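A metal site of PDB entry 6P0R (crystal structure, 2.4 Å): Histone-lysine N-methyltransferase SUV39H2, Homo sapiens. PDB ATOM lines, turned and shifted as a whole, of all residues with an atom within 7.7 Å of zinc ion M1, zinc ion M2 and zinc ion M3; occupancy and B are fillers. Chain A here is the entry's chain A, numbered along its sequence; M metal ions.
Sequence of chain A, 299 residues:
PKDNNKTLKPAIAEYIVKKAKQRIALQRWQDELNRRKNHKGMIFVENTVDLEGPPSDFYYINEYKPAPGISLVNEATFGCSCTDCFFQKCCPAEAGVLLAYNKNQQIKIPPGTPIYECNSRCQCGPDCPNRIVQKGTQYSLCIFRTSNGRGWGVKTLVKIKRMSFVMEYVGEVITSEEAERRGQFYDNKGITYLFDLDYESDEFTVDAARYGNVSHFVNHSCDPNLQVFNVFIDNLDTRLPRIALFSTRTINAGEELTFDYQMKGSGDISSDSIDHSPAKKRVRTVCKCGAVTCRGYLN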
ATOM      1  N   PHE A  78     -30.457  -2.182   8.984  1.00  0.00           N
ATOM      2  CA  PHE A  78     -29.725  -1.233   9.828  1.00  0.00           C
ATOM      3  C   PHE A  78     -28.232  -1.195   9.501  1.00  0.00           C
ATOM      4  O   PHE A  78     -27.621  -2.220   9.192  1.00  0.00           O
ATOM      5  CB  PHE A  78     -29.886  -1.580  11.316  1.00  0.00           C
ATOM      6  CG  PHE A  78     -31.270  -1.341  11.840  1.00  0.00           C
ATOM      7  CD1 PHE A  78     -31.746  -0.041  12.008  1.00  0.00           C
ATOM      8  CD2 PHE A  78     -32.113  -2.418  12.159  1.00  0.00           C
ATOM      9  CE1 PHE A  78     -33.040   0.194  12.484  1.00  0.00           C
ATOM     10  CE2 PHE A  78     -33.395  -2.187  12.648  1.00  0.00           C
ATOM     11  CZ  PHE A  78     -33.862  -0.891  12.814  1.00  0.00           C
ATOM     12  N   GLY A  79     -27.663   0.003   9.567  1.00  0.00           N
ATOM     13  CA  GLY A  79     -26.233   0.216   9.396  1.00  0.00           C
ATOM     14  C   GLY A  79     -25.686   0.983  10.578  1.00  0.00           C
ATOM     15  O   GLY A  79     -26.345   1.085  11.617  1.00  0.00           O
ATOM     16  N   CYS A  80     -24.487   1.491  10.424  1.00  0.00           N
ATOM     17  CA  CYS A  80     -23.832   2.274  11.469  1.00  0.00           C
ATOM     18  C   CYS A  80     -24.147   3.729  11.296  1.00  0.00           C
ATOM     19  O   CYS A  80     -24.699   4.131  10.269  1.00  0.00           O
ATOM     20  CB  CYS A  80     -22.334   2.081  11.415  1.00  0.00           C
ATOM     21  SG  CYS A  80     -21.546   2.613   9.871  1.00  0.00           S
ATOM     22  N   SER A  81     -23.804   4.524  12.300  1.00  0.00           N
ATOM     23  CA  SER A  81     -23.949   5.963  12.266  1.00  0.00           C
ATOM     24  C   SER A  81     -22.624   6.677  12.621  1.00  0.00           C
ATOM     25  O   SER A  81     -22.635   7.823  13.097  1.00  0.00           O
ATOM     26  CB  SER A  81     -25.046   6.419  13.240  1.00  0.00           C
ATOM     27  OG  SER A  81     -26.191   5.591  13.172  1.00  0.00           O
ATOM     28  N   CYS A  82     -21.471   6.002  12.370  1.00  0.00           N
ATOM     29  CA  CYS A  82     -20.164   6.625  12.582  1.00  0.00           C
ATOM     30  C   CYS A  82     -20.003   7.855  11.693  1.00  0.00           C
ATOM     31  O   CYS A  82     -20.559   7.908  10.580  1.00  0.00           O
ATOM     32  CB  CYS A  82     -18.990   5.652  12.257  1.00  0.00           C
ATOM     33  SG  CYS A  82     -19.244   3.914  12.578  1.00  0.00           S
ATOM     34  N   THR A  83     -19.239   8.830  12.169  1.00  0.00           N
ATOM     35  CA  THR A  83     -18.674   9.867  11.303  1.00  0.00           C
ATOM     36  C   THR A  83     -17.268   9.449  10.800  1.00  0.00           C
ATOM     37  O   THR A  83     -16.847   9.868   9.720  1.00  0.00           O
ATOM     38  CB  THR A  83     -18.627  11.237  12.012  1.00  0.00           C
ATOM     39  OG1 THR A  83     -17.894  11.126  13.227  1.00  0.00           O
ATOM     40  CG2 THR A  83     -20.037  11.711  12.331  1.00  0.00           C
ATOM     41  N   ASP A  84     -16.564   8.623  11.603  1.00  0.00           N
ATOM     42  CA  ASP A  84     -15.278   7.992  11.220  1.00  0.00           C
ATOM     43  C   ASP A  84     -15.362   6.468  11.449  1.00  0.00           C
ATOM     44  O   ASP A  84     -15.156   5.982  12.559  1.00  0.00           O
ATOM     45  CB  ASP A  84     -14.114   8.580  12.052  1.00  0.00           C
ATOM     46  CG  ASP A  84     -12.730   8.036  11.621  1.00  0.00           C
ATOM     47  OD1 ASP A  84     -12.641   6.863  11.154  1.00  0.00           O
ATOM     48  OD2 ASP A  84     -11.731   8.761  11.765  1.00  0.00           O
ATOM     49  N   CYS A  85     -15.638   5.726  10.372  1.00  0.00           N
ATOM     50  CA  CYS A  85     -15.849   4.277  10.485  1.00  0.00           C
ATOM     51  C   CYS A  85     -14.589   3.471  10.816  1.00  0.00           C
ATOM     52  O   CYS A  85     -14.691   2.311  11.234  1.00  0.00           O
ATOM     53  CB  CYS A  85     -16.473   3.741   9.205  1.00  0.00           C
ATOM     54  SG  CYS A  85     -18.203   4.172   9.005  1.00  0.00           S
ATOM     55  N   PHE A  86     -13.414   4.065  10.611  1.00  0.00           N
ATOM     56  CA  PHE A  86     -12.150   3.405  10.966  1.00  0.00           C
ATOM     57  C   PHE A  86     -11.939   3.383  12.486  1.00  0.00           C
ATOM     58  O   PHE A  86     -11.597   2.350  13.050  1.00  0.00           O
ATOM     59  CB  PHE A  86     -10.959   4.104  10.268  1.00  0.00           C
ATOM     60  CG  PHE A  86      -9.647   3.408  10.465  1.00  0.00           C
ATOM     61  CD1 PHE A  86      -9.335   2.251   9.752  1.00  0.00           C
ATOM     62  CD2 PHE A  86      -8.708   3.913  11.370  1.00  0.00           C
ATOM     63  CE1 PHE A  86      -8.122   1.607   9.943  1.00  0.00           C
ATOM     64  CE2 PHE A  86      -7.483   3.272  11.567  1.00  0.00           C
ATOM     65  CZ  PHE A  86      -7.196   2.109  10.843  1.00  0.00           C
ATOM     66  N   GLN A  88     -14.338   4.445  14.960  1.00  0.00           N
ATOM     67  CA  GLN A  88     -15.537   4.164  15.761  1.00  0.00           C
ATOM     68  C   GLN A  88     -15.947   2.686  15.673  1.00  0.00           C
ATOM     69  O   GLN A  88     -15.647   2.010  14.694  1.00  0.00           O
ATOM     70  CB  GLN A  88     -16.689   5.049  15.323  1.00  0.00           C
ATOM     71  CG  GLN A  88     -16.449   6.523  15.542  1.00  0.00           C
ATOM     72  CD  GLN A  88     -17.690   7.347  15.288  1.00  0.00           C
ATOM     73  OE1 GLN A  88     -17.773   8.093  14.294  1.00  0.00           O
ATOM     74  NE2 GLN A  88     -18.689   7.213  16.164  1.00  0.00           N
ATOM     75  N   LYS A  89     -16.630   2.211  16.718  1.00  0.00           N
ATOM     76  CA  LYS A  89     -17.239   0.879  16.712  1.00  0.00           C
ATOM     77  C   LYS A  89     -18.323   0.896  15.653  1.00  0.00           C
ATOM     78  O   LYS A  89     -19.303   1.635  15.759  1.00  0.00           O
ATOM     79  CB  LYS A  89     -17.820   0.496  18.087  1.00  0.00           C
ATOM     80  CG  LYS A  89     -16.791  -0.034  19.064  1.00  0.00           C
ATOM     81  CD  LYS A  89     -17.334  -0.146  20.475  1.00  0.00           C
ATOM     82  CE  LYS A  89     -18.377  -1.258  20.601  1.00  0.00           C
ATOM     83  NZ  LYS A  89     -18.594  -1.660  22.023  1.00  0.00           N
ATOM     84  N   CYS A  90     -18.138   0.045  14.650  1.00  0.00           N
ATOM     85  CA  CYS A  90     -18.789   0.187  13.375  1.00  0.00           C
ATOM     86  C   CYS A  90     -19.544  -1.124  13.076  1.00  0.00           C
ATOM     87  O   CYS A  90     -19.768  -1.931  13.976  1.00  0.00           O
ATOM     88  CB  CYS A  90     -17.705   0.493  12.333  1.00  0.00           C
ATOM     89  SG  CYS A  90     -18.240   0.814  10.645  1.00  0.00           S
ATOM     90  N   CYS A  91     -19.960  -1.302  11.817  1.00  0.00           N
ATOM     91  CA  CYS A  91     -20.668  -2.532  11.370  1.00  0.00           C
ATOM     92  C   CYS A  91     -20.003  -3.850  11.839  1.00  0.00           C
ATOM     93  O   CYS A  91     -20.688  -4.724  12.382  1.00  0.00           O
ATOM     94  CB  CYS A  91     -20.890  -2.505   9.837  1.00  0.00           C
ATOM     95  SG  CYS A  91     -22.174  -1.327   9.275  1.00  0.00           S
ATOM     96  N   PRO A  92     -18.651  -3.990  11.685  1.00  0.00           N
ATOM     97  CA  PRO A  92     -17.947  -5.201  12.166  1.00  0.00           C
ATOM     98  C   PRO A  92     -18.123  -5.464  13.671  1.00  0.00           C
ATOM     99  O   PRO A  92     -18.420  -6.608  14.068  1.00  0.00           O
ATOM    100  CB  PRO A  92     -16.474  -4.914  11.840  1.00  0.00           C
ATOM    101  CG  PRO A  92     -16.498  -3.888  10.772  1.00  0.00           C
ATOM    102  CD  PRO A  92     -17.709  -3.048  11.035  1.00  0.00           C
ATOM    103  N   TYR A 116     -17.433  -7.706   7.237  1.00  0.00           N
ATOM    104  CA  TYR A 116     -18.697  -7.004   7.333  1.00  0.00           C
ATOM    105  C   TYR A 116     -18.482  -5.569   6.919  1.00  0.00           C
ATOM    106  O   TYR A 116     -17.910  -4.770   7.669  1.00  0.00           O
ATOM    107  CB  TYR A 116     -19.276  -7.100   8.749  1.00  0.00           C
ATOM    108  CG  TYR A 116     -19.991  -8.413   9.009  1.00  0.00           C
ATOM    109  CD1 TYR A 116     -19.304  -9.533   9.472  1.00  0.00           C
ATOM    110  CD2 TYR A 116     -21.373  -8.532   8.782  1.00  0.00           C
ATOM    111  CE1 TYR A 116     -19.960 -10.734   9.712  1.00  0.00           C
ATOM    112  CE2 TYR A 116     -22.047  -9.725   9.025  1.00  0.00           C
ATOM    113  CZ  TYR A 116     -21.335 -10.833   9.477  1.00  0.00           C
ATOM    114  OH  TYR A 116     -22.000 -12.029   9.718  1.00  0.00           O
ATOM    115  N   GLU A 117     -18.914  -5.251   5.694  1.00  0.00           N
ATOM    116  CA  GLU A 117     -18.770  -3.906   5.153  1.00  0.00           C
ATOM    117  C   GLU A 117     -19.971  -3.092   5.478  1.00  0.00           C
ATOM    118  O   GLU A 117     -21.017  -3.628   5.852  1.00  0.00           O
ATOM    119  CB  GLU A 117     -18.562  -3.937   3.636  1.00  0.00           C
ATOM    120  CG  GLU A 117     -17.308  -4.718   3.204  1.00  0.00           C
ATOM    121  CD  GLU A 117     -16.744  -4.288   1.868  1.00  0.00           C
ATOM    122  OE1 GLU A 117     -17.412  -3.545   1.108  1.00  0.00           O
ATOM    123  OE2 GLU A 117     -15.597  -4.691   1.574  1.00  0.00           O
ATOM    124  N   CYS A 118     -19.810  -1.776   5.355  1.00  0.00           N
ATOM    125  CA  CYS A 118     -20.916  -0.835   5.419  1.00  0.00           C
ATOM    126  C   CYS A 118     -21.805  -1.027   4.220  1.00  0.00           C
ATOM    127  O   CYS A 118     -21.354  -1.516   3.173  1.00  0.00           O
ATOM    128  CB  CYS A 118     -20.380   0.593   5.466  1.00  0.00           C
ATOM    129  SG  CYS A 118     -19.635   0.955   7.032  1.00  0.00           S
ATOM    130  N   ASN A 119     -23.061  -0.620   4.366  1.00  0.00           N
ATOM    131  CA  ASN A 119     -24.130  -0.984   3.432  1.00  0.00           C
ATOM    132  C   ASN A 119     -25.001   0.246   3.105  1.00  0.00           C
ATOM    133  O   ASN A 119     -24.647   1.358   3.464  1.00  0.00           O
ATOM    134  CB  ASN A 119     -24.944  -2.179   3.994  1.00  0.00           C
ATOM    135  CG  ASN A 119     -25.521  -1.913   5.383  1.00  0.00           C
ATOM    136  OD1 ASN A 119     -26.376  -1.064   5.552  1.00  0.00           O
ATOM    137  ND2 ASN A 119     -25.043  -2.670   6.384  1.00  0.00           N
ATOM    138  N   ARG A 121     -27.777   1.167   4.322  1.00  0.00           N
ATOM    139  CA  ARG A 121     -28.444   1.696   5.500  1.00  0.00           C
ATOM    140  C   ARG A 121     -27.483   2.463   6.430  1.00  0.00           C
ATOM    141  O   ARG A 121     -27.921   3.090   7.371  1.00  0.00           O
ATOM    142  CB  ARG A 121     -29.123   0.551   6.294  1.00  0.00           C
ATOM    143  CG  ARG A 121     -29.907  -0.461   5.434  1.00  0.00           C
ATOM    144  CD  ARG A 121     -31.398  -0.154   5.347  1.00  0.00           C
ATOM    145  NE  ARG A 121     -31.705   1.219   4.963  1.00  0.00           N
ATOM    146  CZ  ARG A 121     -31.828   1.670   3.705  1.00  0.00           C
ATOM    147  NH1 ARG A 121     -32.099   2.964   3.493  1.00  0.00           N
ATOM    148  NH2 ARG A 121     -31.670   0.852   2.643  1.00  0.00           N
ATOM    149  N   CYS A 122     -26.163   2.387   6.161  1.00  0.00           N
ATOM    150  CA  CYS A 122     -25.168   3.163   6.928  1.00  0.00           C
ATOM    151  C   CYS A 122     -25.212   4.619   6.495  1.00  0.00           C
ATOM    152  O   CYS A 122     -25.596   4.912   5.370  1.00  0.00           O
ATOM    153  CB  CYS A 122     -23.752   2.607   6.742  1.00  0.00           C
ATOM    154  SG  CYS A 122     -23.445   0.934   7.362  1.00  0.00           S
ATOM    155  N   GLN A 123     -24.788   5.512   7.375  1.00  0.00           N
ATOM    156  CA  GLN A 123     -24.753   6.954   7.073  1.00  0.00           C
ATOM    157  C   GLN A 123     -23.541   7.367   6.258  1.00  0.00           C
ATOM    158  O   GLN A 123     -23.601   8.336   5.488  1.00  0.00           O
ATOM    159  CB  GLN A 123     -24.810   7.791   8.371  1.00  0.00           C
ATOM    160  CG  GLN A 123     -26.058   7.557   9.216  1.00  0.00           C
ATOM    161  CD  GLN A 123     -27.342   7.798   8.433  1.00  0.00           C
ATOM    162  OE1 GLN A 123     -27.443   8.763   7.690  1.00  0.00           O
ATOM    163  NE2 GLN A 123     -28.310   6.894   8.588  1.00  0.00           N
ATOM    164  N   CYS A 124     -22.427   6.658   6.434  1.00  0.00           N
ATOM    165  CA  CYS A 124     -21.173   6.997   5.754  1.00  0.00           C
ATOM    166  C   CYS A 124     -21.280   6.964   4.211  1.00  0.00           C
ATOM    167  O   CYS A 124     -22.042   6.148   3.645  1.00  0.00           O
ATOM    168  CB  CYS A 124     -20.057   6.067   6.225  1.00  0.00           C
ATOM    169  SG  CYS A 124     -20.397   4.322   5.857  1.00  0.00           S
ATOM    170  N   GLY A 125     -20.539   7.855   3.546  1.00  0.00           N
ATOM    171  CA  GLY A 125     -20.483   7.916   2.075  1.00  0.00           C
ATOM    172  C   GLY A 125     -19.549   6.875   1.461  1.00  0.00           C
ATOM    173  O   GLY A 125     -18.986   6.037   2.177  1.00  0.00           O
ATOM    174  N   ASP A 127     -16.551   7.030   0.207  1.00  0.00           N
ATOM    175  CA  ASP A 127     -15.162   7.142   0.718  1.00  0.00           C
ATOM    176  C   ASP A 127     -14.872   6.436   2.076  1.00  0.00           C
ATOM    177  O   ASP A 127     -13.733   6.471   2.549  1.00  0.00           O
ATOM    178  CB  ASP A 127     -14.708   8.630   0.771  1.00  0.00           C
ATOM    179  CG  ASP A 127     -15.738   9.547   1.481  1.00  0.00           C
ATOM    180  OD1 ASP A 127     -16.911   9.598   1.036  1.00  0.00           O
ATOM    181  OD2 ASP A 127     -15.340  10.231   2.439  1.00  0.00           O
ATOM    182  N   CYS A 128     -15.891   5.805   2.687  1.00  0.00           N
ATOM    183  CA  CYS A 128     -15.702   4.998   3.900  1.00  0.00           C
ATOM    184  C   CYS A 128     -14.663   3.888   3.677  1.00  0.00           C
ATOM    185  O   CYS A 128     -14.756   3.176   2.689  1.00  0.00           O
ATOM    186  CB  CYS A 128     -17.043   4.371   4.349  1.00  0.00           C
ATOM    187  SG  CYS A 128     -16.889   3.145   5.694  1.00  0.00           S
ATOM    188  N   PRO A 129     -13.678   3.746   4.597  1.00  0.00           N
ATOM    189  CA  PRO A 129     -12.639   2.716   4.433  1.00  0.00           C
ATOM    190  C   PRO A 129     -13.117   1.273   4.663  1.00  0.00           C
ATOM    191  O   PRO A 129     -12.369   0.351   4.372  1.00  0.00           O
ATOM    192  CB  PRO A 129     -11.582   3.112   5.477  1.00  0.00           C
ATOM    193  CG  PRO A 129     -12.344   3.818   6.530  1.00  0.00           C
ATOM    194  CD  PRO A 129     -13.450   4.555   5.818  1.00  0.00           C
ATOM    195  N   ASN A 130     -14.335   1.091   5.191  1.00  0.00           N
ATOM    196  CA  ASN A 130     -15.023  -0.206   5.211  1.00  0.00           C
ATOM    197  C   ASN A 130     -15.989  -0.417   4.002  1.00  0.00           C
ATOM    198  O   ASN A 130     -16.907  -1.231   4.072  1.00  0.00           O
ATOM    199  CB  ASN A 130     -15.807  -0.361   6.549  1.00  0.00           C
ATOM    200  CG  ASN A 130     -16.107  -1.816   6.896  1.00  0.00           C
ATOM    201  OD1 ASN A 130     -15.348  -2.722   6.554  1.00  0.00           O
ATOM    202  ND2 ASN A 130     -17.225  -2.035   7.608  1.00  0.00           N
ATOM    203  N   ARG A 131     -15.785   0.337   2.910  1.00  0.00           N
ATOM    204  CA  ARG A 131     -16.507   0.123   1.637  1.00  0.00           C
ATOM    205  C   ARG A 131     -15.499  -0.183   0.514  1.00  0.00           C
ATOM    206  O   ARG A 131     -15.099   0.716  -0.231  1.00  0.00           O
ATOM    207  CB  ARG A 131     -17.358   1.358   1.278  1.00  0.00           C
ATOM    208  CG  ARG A 131     -18.576   1.600   2.151  1.00  0.00           C
ATOM    209  CD  ARG A 131     -19.356   2.781   1.623  1.00  0.00           C
ATOM    210  NE  ARG A 131     -20.465   3.222   2.485  1.00  0.00           N
ATOM    211  CZ  ARG A 131     -21.698   2.685   2.506  1.00  0.00           C
ATOM    212  NH1 ARG A 131     -21.994   1.609   1.768  1.00  0.00           N
ATOM    213  NH2 ARG A 131     -22.633   3.216   3.302  1.00  0.00           N
HETATM  214 ZN    ZN M   1     -19.367   2.854  10.536  1.00  0.00          ZN
HETATM  215 ZN    ZN M   2     -21.439   0.739   8.536  1.00  0.00          ZN
HETATM  216 ZN    ZN M   3     -18.824   3.135   7.035  1.00  0.00          ZN
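The side-chain sulfur (SG) of Cys 122 sits close to the backbone NH (N) of Asn 119 (3.4 Å).
O of Cys 118 is in hydrogen-bond range of NH1 of Arg 131 (3.5 Å).
The backbone carbonyl oxygen (O) of Cys 80 sits at hydrogen-bond distance from the backbone NH (N) of Gln 123, 3.2 Å away.
N of Asn 130 lies close to SG of Cys 128 (3.3 Å).
N of Cys 118 is in hydrogen-bond range of O of Asn 130, 3.2 Å away.
NH2 of Arg 131 lies within hydrogen-bond range of O of Cys 124 (3.0 Å).
Five residues have an atom within 4 Å of zinc ion M1: Cys 80, Cys 82, Cys 85, Cys 90 and Cys 118.
Zinc ion M3 is bound by SG of Cys 124 (2.3 Å), SG of Cys 85 (2.3 Å), SG of Cys 118 (2.3 Å) and SG of Cys 128 (2.4 Å).
Zinc ion M3 has four donor atoms within binding distance.
The nearest printed residue that does not touch zinc ion M3 is Cys 90 (4.3 Å).
Zinc ion M1 is bound by the side-chain sulfur of Cys 80 (2.3 Å), the side-chain sulfur of Cys 82 (2.3 Å), the side-chain sulfur of Cys 85 (2.3 Å) and the side-chain sulfur of Cys 90 (2.3 Å).
Within 4 Å of zinc ion M2: Cys 80, Cys 90, Cys 91, Cys 118 and Cys 122.
The nearest printed residue that does not touch zinc ion M2 is Cys 124 (4.6 Å).
Zinc ion M2 is bound by SG of Cys 80 (2.3 Å), SG of Cys 91 (2.3 Å), SG of Cys 122 (2.3 Å) and SG of Cys 118 (2.4 Å).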
